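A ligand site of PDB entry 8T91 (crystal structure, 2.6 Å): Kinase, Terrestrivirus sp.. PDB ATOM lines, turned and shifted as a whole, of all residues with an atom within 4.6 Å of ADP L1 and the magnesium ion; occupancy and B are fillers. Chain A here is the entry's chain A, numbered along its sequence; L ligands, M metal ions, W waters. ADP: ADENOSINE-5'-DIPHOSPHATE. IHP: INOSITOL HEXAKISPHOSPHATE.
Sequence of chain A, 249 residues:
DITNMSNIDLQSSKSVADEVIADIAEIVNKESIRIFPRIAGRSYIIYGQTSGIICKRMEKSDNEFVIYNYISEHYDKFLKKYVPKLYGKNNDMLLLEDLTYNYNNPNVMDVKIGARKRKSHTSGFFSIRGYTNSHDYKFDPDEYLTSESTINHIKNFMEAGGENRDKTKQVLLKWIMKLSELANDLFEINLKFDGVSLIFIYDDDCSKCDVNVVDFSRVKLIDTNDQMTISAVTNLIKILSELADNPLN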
ATOM      1  N   PHE A  36      10.521   2.427  24.064  1.00  0.00           N
ATOM      2  CA  PHE A  36      11.180   1.156  24.456  1.00  0.00           C
ATOM      3  C   PHE A  36      12.634   1.419  24.831  1.00  0.00           C
ATOM      4  O   PHE A  36      13.349   2.053  24.051  1.00  0.00           O
ATOM      5  CB  PHE A  36      11.120   0.122  23.330  1.00  0.00           C
ATOM      6  CG  PHE A  36      11.604  -1.238  23.733  1.00  0.00           C
ATOM      7  CD1 PHE A  36      10.793  -2.093  24.456  1.00  0.00           C
ATOM      8  CD2 PHE A  36      12.900  -1.648  23.435  1.00  0.00           C
ATOM      9  CE1 PHE A  36      11.246  -3.344  24.847  1.00  0.00           C
ATOM     10  CE2 PHE A  36      13.351  -2.901  23.837  1.00  0.00           C
ATOM     11  CZ  PHE A  36      12.521  -3.750  24.537  1.00  0.00           C
ATOM     12  N   ARG A  38      15.805   0.874  24.402  1.00  0.00           N
ATOM     13  CA  ARG A  38      16.892   0.387  23.508  1.00  0.00           C
ATOM     14  C   ARG A  38      18.219   0.412  24.280  1.00  0.00           C
ATOM     15  O   ARG A  38      18.445   1.353  25.048  1.00  0.00           O
ATOM     16  CB  ARG A  38      17.034   1.281  22.270  1.00  0.00           C
ATOM     17  CG  ARG A  38      15.900   1.146  21.262  1.00  0.00           C
ATOM     18  CD  ARG A  38      15.673   2.452  20.518  1.00  0.00           C
ATOM     19  NE  ARG A  38      16.919   2.985  19.977  1.00  0.00           N
ATOM     20  CZ  ARG A  38      17.224   4.278  19.830  1.00  0.00           C
ATOM     21  NH1 ARG A  38      16.359   5.223  20.178  1.00  0.00           N
ATOM     22  NH2 ARG A  38      18.385   4.625  19.322  1.00  0.00           N
ATOM     23  N   ILE A  39      19.069  -0.594  24.072  1.00  0.00           N
ATOM     24  CA  ILE A  39      20.449  -0.626  24.643  1.00  0.00           C
ATOM     25  C   ILE A  39      21.385   0.062  23.645  1.00  0.00           C
ATOM     26  O   ILE A  39      22.340   0.699  24.098  1.00  0.00           O
ATOM     27  CB  ILE A  39      20.887  -2.067  25.004  1.00  0.00           C
ATOM     28  CG1 ILE A  39      21.206  -2.200  26.496  1.00  0.00           C
ATOM     29  CG2 ILE A  39      22.065  -2.531  24.156  1.00  0.00           C
ATOM     30  CD1 ILE A  39      20.103  -1.769  27.419  1.00  0.00           C
ATOM     31  N   ALA A  40      21.119  -0.052  22.334  1.00  0.00           N
ATOM     32  CA  ALA A  40      21.985   0.495  21.257  1.00  0.00           C
ATOM     33  C   ALA A  40      21.147   0.858  20.017  1.00  0.00           C
ATOM     34  O   ALA A  40      19.907   0.977  20.138  1.00  0.00           O
ATOM     35  CB  ALA A  40      23.066  -0.500  20.924  1.00  0.00           C
ATOM     36  N   GLY A  41      21.816   1.030  18.879  1.00  0.00           N
ATOM     37  CA  GLY A  41      21.181   1.401  17.594  1.00  0.00           C
ATOM     38  C   GLY A  41      20.816   2.863  17.585  1.00  0.00           C
ATOM     39  O   GLY A  41      21.230   3.587  18.516  1.00  0.00           O
ATOM     40  N   ARG A  42      20.043   3.295  16.584  1.00  0.00           N
ATOM     41  CA  ARG A  42      19.616   4.703  16.392  1.00  0.00           C
ATOM     42  C   ARG A  42      18.170   4.765  15.870  1.00  0.00           C
ATOM     43  O   ARG A  42      17.736   5.877  15.503  1.00  0.00           O
ATOM     44  CB  ARG A  42      20.659   5.400  15.501  1.00  0.00           C
ATOM     45  CG  ARG A  42      21.867   5.901  16.275  1.00  0.00           C
ATOM     46  CD  ARG A  42      23.211   5.403  15.759  1.00  0.00           C
ATOM     47  NE  ARG A  42      24.166   6.495  15.628  1.00  0.00           N
ATOM     48  CZ  ARG A  42      25.504   6.378  15.560  1.00  0.00           C
ATOM     49  NH1 ARG A  42      26.254   7.455  15.442  1.00  0.00           N
ATOM     50  NH2 ARG A  42      26.086   5.188  15.630  1.00  0.00           N
ATOM     51  N   SER A  43      17.432   3.651  15.899  1.00  0.00           N
ATOM     52  CA  SER A  43      16.067   3.493  15.310  1.00  0.00           C
ATOM     53  C   SER A  43      14.992   3.890  16.322  1.00  0.00           C
ATOM     54  O   SER A  43      15.160   3.624  17.531  1.00  0.00           O
ATOM     55  CB  SER A  43      15.831   2.086  14.815  1.00  0.00           C
ATOM     56  OG  SER A  43      16.584   1.804  13.644  1.00  0.00           O
ATOM     57  N   ILE A  45      12.038   2.927  18.212  1.00  0.00           N
ATOM     58  CA  ILE A  45      11.415   1.669  18.719  1.00  0.00           C
ATOM     59  C   ILE A  45      10.571   2.013  19.943  1.00  0.00           C
ATOM     60  O   ILE A  45      11.121   2.533  20.940  1.00  0.00           O
ATOM     61  CB  ILE A  45      12.432   0.557  19.033  1.00  0.00           C
ATOM     62  CG1 ILE A  45      13.274   0.190  17.804  1.00  0.00           C
ATOM     63  CG2 ILE A  45      11.722  -0.661  19.610  1.00  0.00           C
ATOM     64  CD1 ILE A  45      14.456  -0.726  18.107  1.00  0.00           C
ATOM     65  N   ILE A  54       7.124  -5.055  20.219  1.00  0.00           N
ATOM     66  CA  ILE A  54       7.796  -3.750  19.975  1.00  0.00           C
ATOM     67  C   ILE A  54       7.588  -3.417  18.507  1.00  0.00           C
ATOM     68  O   ILE A  54       7.523  -4.343  17.669  1.00  0.00           O
ATOM     69  CB  ILE A  54       9.283  -3.776  20.386  1.00  0.00           C
ATOM     70  CG1 ILE A  54      10.042  -4.932  19.745  1.00  0.00           C
ATOM     71  CG2 ILE A  54       9.413  -3.775  21.893  1.00  0.00           C
ATOM     72  CD1 ILE A  54      11.533  -4.702  19.582  1.00  0.00           C
ATOM     73  N   LYS A  56       9.327  -1.281  15.489  1.00  0.00           N
ATOM     74  CA  LYS A  56      10.604  -0.721  15.009  1.00  0.00           C
ATOM     75  C   LYS A  56      10.364  -0.065  13.645  1.00  0.00           C
ATOM     76  O   LYS A  56       9.964  -0.772  12.720  1.00  0.00           O
ATOM     77  CB  LYS A  56      11.679  -1.807  14.883  1.00  0.00           C
ATOM     78  CG  LYS A  56      12.892  -1.378  14.070  1.00  0.00           C
ATOM     79  CD  LYS A  56      14.072  -2.321  14.110  1.00  0.00           C
ATOM     80  CE  LYS A  56      15.276  -1.699  13.438  1.00  0.00           C
ATOM     81  NZ  LYS A  56      16.271  -2.706  13.011  1.00  0.00           N
ATOM     82  N   PRO A  84      13.843 -13.128  16.551  1.00  0.00           N
ATOM     83  CA  PRO A  84      12.560 -12.791  17.144  1.00  0.00           C
ATOM     84  C   PRO A  84      11.493 -12.919  16.063  1.00  0.00           C
ATOM     85  O   PRO A  84      11.767 -12.632  14.911  1.00  0.00           O
ATOM     86  CB  PRO A  84      12.730 -11.343  17.609  1.00  0.00           C
ATOM     87  CG  PRO A  84      13.841 -10.816  16.722  1.00  0.00           C
ATOM     88  CD  PRO A  84      14.778 -11.993  16.591  1.00  0.00           C
ATOM     89  N   LEU A  96       7.470  -6.709  16.113  1.00  0.00           N
ATOM     90  CA  LEU A  96       8.503  -7.721  16.470  1.00  0.00           C
ATOM     91  C   LEU A  96       8.247  -8.239  17.885  1.00  0.00           C
ATOM     92  O   LEU A  96       7.783  -7.449  18.733  1.00  0.00           O
ATOM     93  CB  LEU A  96       9.884  -7.059  16.405  1.00  0.00           C
ATOM     94  CG  LEU A  96      10.431  -6.779  15.007  1.00  0.00           C
ATOM     95  CD1 LEU A  96      11.765  -6.050  15.093  1.00  0.00           C
ATOM     96  CD2 LEU A  96      10.595  -8.076  14.223  1.00  0.00           C
ATOM     97  N   GLU A  97       8.554  -9.508  18.112  1.00  0.00           N
ATOM     98  CA  GLU A  97       8.519 -10.128  19.460  1.00  0.00           C
ATOM     99  C   GLU A  97       9.482  -9.356  20.353  1.00  0.00           C
ATOM    100  O   GLU A  97      10.618  -9.120  19.923  1.00  0.00           O
ATOM    101  CB  GLU A  97       8.872 -11.612  19.359  1.00  0.00           C
ATOM    102  CG  GLU A  97       9.259 -12.251  20.672  1.00  0.00           C
ATOM    103  CD  GLU A  97       9.913 -13.603  20.502  1.00  0.00           C
ATOM    104  OE1 GLU A  97      10.033 -14.088  19.336  1.00  0.00           O
ATOM    105  OE2 GLU A  97      10.330 -14.174  21.534  1.00  0.00           O
ATOM    106  N   ASP A  98       9.006  -8.940  21.523  1.00  0.00           N
ATOM    107  CA  ASP A  98       9.832  -8.284  22.562  1.00  0.00           C
ATOM    108  C   ASP A  98      10.598  -9.373  23.303  1.00  0.00           C
ATOM    109  O   ASP A  98       9.970 -10.112  24.081  1.00  0.00           O
ATOM    110  CB  ASP A  98       8.985  -7.447  23.517  1.00  0.00           C
ATOM    111  CG  ASP A  98       9.808  -6.776  24.599  1.00  0.00           C
ATOM    112  OD1 ASP A  98      11.039  -6.962  24.597  1.00  0.00           O
ATOM    113  OD2 ASP A  98       9.200  -6.056  25.426  1.00  0.00           O
ATOM    114  N   LEU A  99      11.913  -9.431  23.069  1.00  0.00           N
ATOM    115  CA  LEU A  99      12.835 -10.475  23.602  1.00  0.00           C
ATOM    116  C   LEU A  99      12.984 -10.311  25.115  1.00  0.00           C
ATOM    117  O   LEU A  99      13.447 -11.275  25.742  1.00  0.00           O
ATOM    118  CB  LEU A  99      14.196 -10.331  22.902  1.00  0.00           C
ATOM    119  CG  LEU A  99      14.189 -10.667  21.412  1.00  0.00           C
ATOM    120  CD1 LEU A  99      15.543 -10.383  20.792  1.00  0.00           C
ATOM    121  CD2 LEU A  99      13.786 -12.123  21.185  1.00  0.00           C
ATOM    122  N   THR A 100      12.600  -9.164  25.666  1.00  0.00           N
ATOM    123  CA  THR A 100      12.726  -8.857  27.113  1.00  0.00           C
ATOM    124  C   THR A 100      11.410  -9.151  27.838  1.00  0.00           C
ATOM    125  O   THR A 100      11.429  -9.033  29.058  1.00  0.00           O
ATOM    126  CB  THR A 100      13.093  -7.392  27.389  1.00  0.00           C
ATOM    127  OG1 THR A 100      11.928  -6.598  27.145  1.00  0.00           O
ATOM    128  CG2 THR A 100      14.278  -6.920  26.571  1.00  0.00           C
ATOM    129  N   VAL A 108      20.430  -6.805  29.314  1.00  0.00           N
ATOM    130  CA  VAL A 108      20.541  -6.892  27.829  1.00  0.00           C
ATOM    131  C   VAL A 108      21.927  -6.416  27.417  1.00  0.00           C
ATOM    132  O   VAL A 108      22.372  -5.373  27.934  1.00  0.00           O
ATOM    133  CB  VAL A 108      19.444  -6.086  27.123  1.00  0.00           C
ATOM    134  CG1 VAL A 108      19.565  -6.185  25.605  1.00  0.00           C
ATOM    135  CG2 VAL A 108      18.064  -6.522  27.585  1.00  0.00           C
ATOM    136  N   ASP A 110      23.920  -5.748  23.621  1.00  0.00           N
ATOM    137  CA  ASP A 110      23.927  -5.694  22.142  1.00  0.00           C
ATOM    138  C   ASP A 110      25.377  -5.849  21.710  1.00  0.00           C
ATOM    139  O   ASP A 110      26.197  -5.005  22.087  1.00  0.00           O
ATOM    140  CB  ASP A 110      23.285  -4.395  21.614  1.00  0.00           C
ATOM    141  CG  ASP A 110      23.195  -4.300  20.100  1.00  0.00           C
ATOM    142  OD1 ASP A 110      24.096  -4.813  19.414  1.00  0.00           O
ATOM    143  OD2 ASP A 110      22.232  -3.669  19.621  1.00  0.00           O
ATOM    144  N   GLY A 195      25.955  -5.707   9.756  1.00  0.00           N
ATOM    145  CA  GLY A 195      25.346  -4.841  10.777  1.00  0.00           C
ATOM    146  C   GLY A 195      24.405  -5.566  11.716  1.00  0.00           C
ATOM    147  O   GLY A 195      23.824  -4.872  12.571  1.00  0.00           O
ATOM    148  N   SER A 197      23.177  -7.777  14.965  1.00  0.00           N
ATOM    149  CA  SER A 197      23.637  -7.856  16.362  1.00  0.00           C
ATOM    150  C   SER A 197      23.120  -9.140  16.990  1.00  0.00           C
ATOM    151  O   SER A 197      22.118  -9.692  16.486  1.00  0.00           O
ATOM    152  CB  SER A 197      23.197  -6.652  17.175  1.00  0.00           C
ATOM    153  OG  SER A 197      24.020  -5.540  16.899  1.00  0.00           O
ATOM    154  N   ILE A 199      21.668 -10.123  20.652  1.00  0.00           N
ATOM    155  CA  ILE A 199      21.031  -9.554  21.865  1.00  0.00           C
ATOM    156  C   ILE A 199      21.087 -10.632  22.934  1.00  0.00           C
ATOM    157  O   ILE A 199      20.228 -11.542  22.877  1.00  0.00           O
ATOM    158  CB  ILE A 199      19.600  -9.115  21.587  1.00  0.00           C
ATOM    159  CG1 ILE A 199      19.549  -8.170  20.389  1.00  0.00           C
ATOM    160  CG2 ILE A 199      18.984  -8.509  22.842  1.00  0.00           C
ATOM    161  CD1 ILE A 199      20.478  -6.986  20.521  1.00  0.00           C
ATOM    162  N   VAL A 214      19.393 -10.007  15.608  1.00  0.00           N
ATOM    163  CA  VAL A 214      18.494  -8.871  15.261  1.00  0.00           C
ATOM    164  C   VAL A 214      19.166  -7.912  14.256  1.00  0.00           C
ATOM    165  O   VAL A 214      20.405  -7.937  14.164  1.00  0.00           O
ATOM    166  CB  VAL A 214      18.036  -8.120  16.524  1.00  0.00           C
ATOM    167  CG1 VAL A 214      17.376  -9.069  17.502  1.00  0.00           C
ATOM    168  CG2 VAL A 214      19.191  -7.368  17.169  1.00  0.00           C
ATOM    169  N   ASP A 215      18.338  -7.102  13.573  1.00  0.00           N
ATOM    170  CA  ASP A 215      18.707  -5.955  12.704  1.00  0.00           C
ATOM    171  C   ASP A 215      19.195  -6.471  11.360  1.00  0.00           C
ATOM    172  O   ASP A 215      20.420  -6.632  11.177  1.00  0.00           O
ATOM    173  CB  ASP A 215      19.733  -5.032  13.369  1.00  0.00           C
ATOM    174  CG  ASP A 215      19.889  -3.680  12.702  1.00  0.00           C
ATOM    175  OD1 ASP A 215      19.265  -3.470  11.631  1.00  0.00           O
ATOM    176  OD2 ASP A 215      20.617  -2.838  13.263  1.00  0.00           O
HETATM  177  PB  ADP L   1      18.973  -0.453  14.854  1.00  0.00           P
HETATM  178  O1B ADP L   1      20.395  -0.752  15.273  1.00  0.00           O
HETATM  179  O2B ADP L   1      18.538   0.914  15.270  1.00  0.00           O
HETATM  180  O3B ADP L   1      18.722  -0.732  13.367  1.00  0.00           O
HETATM  181  PA  ADP L   1      18.292  -2.943  16.322  1.00  0.00           P
HETATM  182  O1A ADP L   1      19.747  -3.309  16.340  1.00  0.00           O
HETATM  183  O2A ADP L   1      17.334  -3.854  15.627  1.00  0.00           O
HETATM  184  O3A ADP L   1      18.063  -1.463  15.727  1.00  0.00           O
HETATM  185  O5' ADP L   1      17.793  -2.722  17.830  1.00  0.00           O
HETATM  186  C5' ADP L   1      18.487  -1.771  18.656  1.00  0.00           C
HETATM  187  C4' ADP L   1      18.225  -2.098  20.099  1.00  0.00           C
HETATM  188  O4' ADP L   1      16.822  -2.432  20.261  1.00  0.00           O
HETATM  189  C3' ADP L   1      18.988  -3.305  20.661  1.00  0.00           C
HETATM  190  O3' ADP L   1      20.205  -2.856  21.231  1.00  0.00           O
HETATM  191  C2' ADP L   1      18.023  -3.870  21.713  1.00  0.00           C
HETATM  192  O2' ADP L   1      18.197  -3.294  22.984  1.00  0.00           O
HETATM  193  C1' ADP L   1      16.644  -3.499  21.160  1.00  0.00           C
HETATM  194  N9  ADP L   1      15.920  -4.548  20.454  1.00  0.00           N
HETATM  195  C8  ADP L   1      15.898  -4.779  19.097  1.00  0.00           C
HETATM  196  N7  ADP L   1      15.106  -5.758  18.747  1.00  0.00           N
HETATM  197  C5  ADP L   1      14.547  -6.199  19.935  1.00  0.00           C
HETATM  198  C6  ADP L   1      13.612  -7.208  20.229  1.00  0.00           C
HETATM  199  N6  ADP L   1      13.039  -7.981  19.311  1.00  0.00           N
HETATM  200  N1  ADP L   1      13.252  -7.356  21.523  1.00  0.00           N
HETATM  201  C2  ADP L   1      13.817  -6.565  22.444  1.00  0.00           C
HETATM  202  N3  ADP L   1      14.716  -5.593  22.292  1.00  0.00           N
HETATM  203  C4  ADP L   1      15.035  -5.451  20.992  1.00  0.00           C
HETATM  204  C1  IHP L   2      25.259   2.632  12.810  1.00  0.00           C
HETATM  205  C2  IHP L   2      24.203   3.182  11.880  1.00  0.00           C
HETATM  206  C3  IHP L   2      24.615   4.669  11.570  1.00  0.00           C
HETATM  207  C4  IHP L   2      26.031   4.762  10.866  1.00  0.00           C
HETATM  208  C5  IHP L   2      27.090   3.981  11.655  1.00  0.00           C
HETATM  209  C6  IHP L   2      26.586   2.595  12.047  1.00  0.00           C
HETATM  210  O11 IHP L   2      24.817   1.337  13.362  1.00  0.00           O
HETATM  211  P1  IHP L   2      24.138   1.284  14.842  1.00  0.00           P
HETATM  212  O21 IHP L   2      25.414   1.441  15.759  1.00  0.00           O
HETATM  213  O31 IHP L   2      23.138   2.510  14.914  1.00  0.00           O
HETATM  214  O41 IHP L   2      23.504  -0.040  14.892  1.00  0.00           O
HETATM  215  O12 IHP L   2      24.080   2.362  10.688  1.00  0.00           O
HETATM  216  P2  IHP L   2      22.643   2.132  10.003  1.00  0.00           P
HETATM  217  O22 IHP L   2      22.409   0.649  10.511  1.00  0.00           O
HETATM  218  O32 IHP L   2      22.820   2.276   8.430  1.00  0.00           O
HETATM  219  O42 IHP L   2      21.760   3.133  10.649  1.00  0.00           O
HETATM  220  O13 IHP L   2      23.592   5.371  10.821  1.00  0.00           O
HETATM  221  P3  IHP L   2      22.772   6.502  11.594  1.00  0.00           P
HETATM  222  O23 IHP L   2      22.012   7.370  10.519  1.00  0.00           O
HETATM  223  O33 IHP L   2      23.961   7.321  12.257  1.00  0.00           O
HETATM  224  O43 IHP L   2      21.990   5.806  12.661  1.00  0.00           O
HETATM  225  O14 IHP L   2      26.481   6.147  10.684  1.00  0.00           O
HETATM  226  P4  IHP L   2      26.749   6.781   9.192  1.00  0.00           P
HETATM  227  O24 IHP L   2      25.373   6.596   8.390  1.00  0.00           O
HETATM  228  O34 IHP L   2      27.820   5.877   8.455  1.00  0.00           O
HETATM  229  O44 IHP L   2      26.989   8.259   9.311  1.00  0.00           O
HETATM  230  O15 IHP L   2      28.256   3.821  10.797  1.00  0.00           O
HETATM  231  P5  IHP L   2      29.754   4.387  11.054  1.00  0.00           P
HETATM  232  O25 IHP L   2      30.565   3.067  10.694  1.00  0.00           O
HETATM  233  O35 IHP L   2      29.813   4.818  12.580  1.00  0.00           O
HETATM  234  O45 IHP L   2      29.963   5.463  10.038  1.00  0.00           O
HETATM  235  O16 IHP L   2      27.564   2.090  12.894  1.00  0.00           O
HETATM  236  P6  IHP L   2      28.356   0.739  12.535  1.00  0.00           P
HETATM  237  O26 IHP L   2      29.748   1.329  12.188  1.00  0.00           O
HETATM  238  O36 IHP L   2      27.750   0.077  11.234  1.00  0.00           O
HETATM  239  O46 IHP L   2      28.459  -0.054  13.823  1.00  0.00           O
HETATM  240 MG    MG M   1      21.475  -2.409  15.296  1.00  0.00          MG
HETATM  241  O   HOH W   1      22.144  -2.372  17.473  1.00  0.00           O
HETATM  242  O   HOH W   2      22.764  -4.385  15.043  1.00  0.00           O
HETATM  243  O   HOH W   3      15.206  -5.414  15.652  1.00  0.00           O
HETATM  244  O   HOH W   4      22.796  -1.967  13.985  1.00  0.00           O
HETATM  245  O   HOH W   5      16.503  -4.462  24.502  1.00  0.00           O
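The backbone NH (N) of Ser 43 sits close to an oxygen (O2B) of ADP L1, at 3.0 Å. The side-chain hydroxyl of Ser 43 lies within hydrogen-bond range of an oxygen (O2B) of ADP L1. OD2 of Asp 110 lies within hydrogen-bond range of O3' of ADP L1 (2.7 Å). A nitrogen (N6) of ADP L1 lies within hydrogen-bond range of the backbone carbonyl oxygen (O) of Glu 97 (2.7 Å). N of Leu 99 is in hydrogen-bond range of N1 of ADP L1 (2.9 Å). The backbone NH (N) of Ile 39 lies within hydrogen-bond range of an oxygen (O2') of ADP L1 (3.0 Å). An oxygen (O2A) of ADP L1 lies within salt-bridge range of the side-chain amino group of Lys 56 (3.0 Å). N of Arg 42 lies within hydrogen-bond range of O2B of ADP L1 (3.1 Å). An oxygen (O3') of ADP L1 lies within hydrogen-bond range of the backbone NH (N) of Ala 40 (3.1 Å). O33 of IHP L2 is in salt-bridge range of NE of Arg 42.
The side-chain amino group (NZ) of Lys 56 is in salt-bridge range of the side-chain carboxylate (OD1) of Asp 215, 3.4 Å away. O of Ser 43 is in hydrogen-bond range of NE of Arg 38 (3.1 Å). The side-chain hydroxyl (OG) of Ser 197 sits at hydrogen-bond distance from the side-chain carboxylate (OD1) of Asp 110, at 2.6 Å. The backbone carbonyl oxygen (O) of Gly 41 is in hydrogen-bond range of the guanidinium group (NH2) of Arg 38. N of Leu 96 lies within hydrogen-bond range of O of Ile 54 (2.8 Å). The backbone carbonyl oxygen (O) of Ile 45 lies within hydrogen-bond range of the backbone NH (N) of Phe 36 (3.2 Å). OD1 of Asp 98 is in hydrogen-bond range of OG1 of Thr 100, at 2.7 Å.
CE2 of Phe 36 touches N3 of ADP L1 (3.4 Å). CG of Arg 38 touches O4' of ADP L1, 3.8 Å away. Gly 41 touches ADP L1 (CA to O1B, 3.3 Å). CD1 of Ile 45 touches O4' of ADP L1 (3.6 Å). CD1 of Ile 54 touches C6 of ADP L1, at 3.3 Å. CB of Pro 84 touches N6 of ADP L1 (3.8 Å). OD1 of Asp 98 touches C2 of ADP L1 (3.5 Å). Ile 199 touches ADP L1. Hydrophobic or aromatic side chains within 4 Å of ADP L1: Phe 36, Ile 39, Ala 40, Ile 45, Ile 54, Pro 84, Leu 99 and Ile 199.
One residue has an atom within 4 Å of the magnesium ion: Asp 215. The nearest printed residue that does not touch the magnesium ion is Ser 197 (4.3 Å).
The magnesium ion is bound by water W4 (1.9 Å), O1B of ADP L1 (2.0 Å), O1A of ADP L1 (2.2 Å), OD2 of Asp 215 (2.2 Å), water W1 (2.3 Å) and water W2 (2.4 Å).
Water W2 bridges the side-chain hydroxyl of Ser 197 and the backbone carbonyl oxygen of Gly 195.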
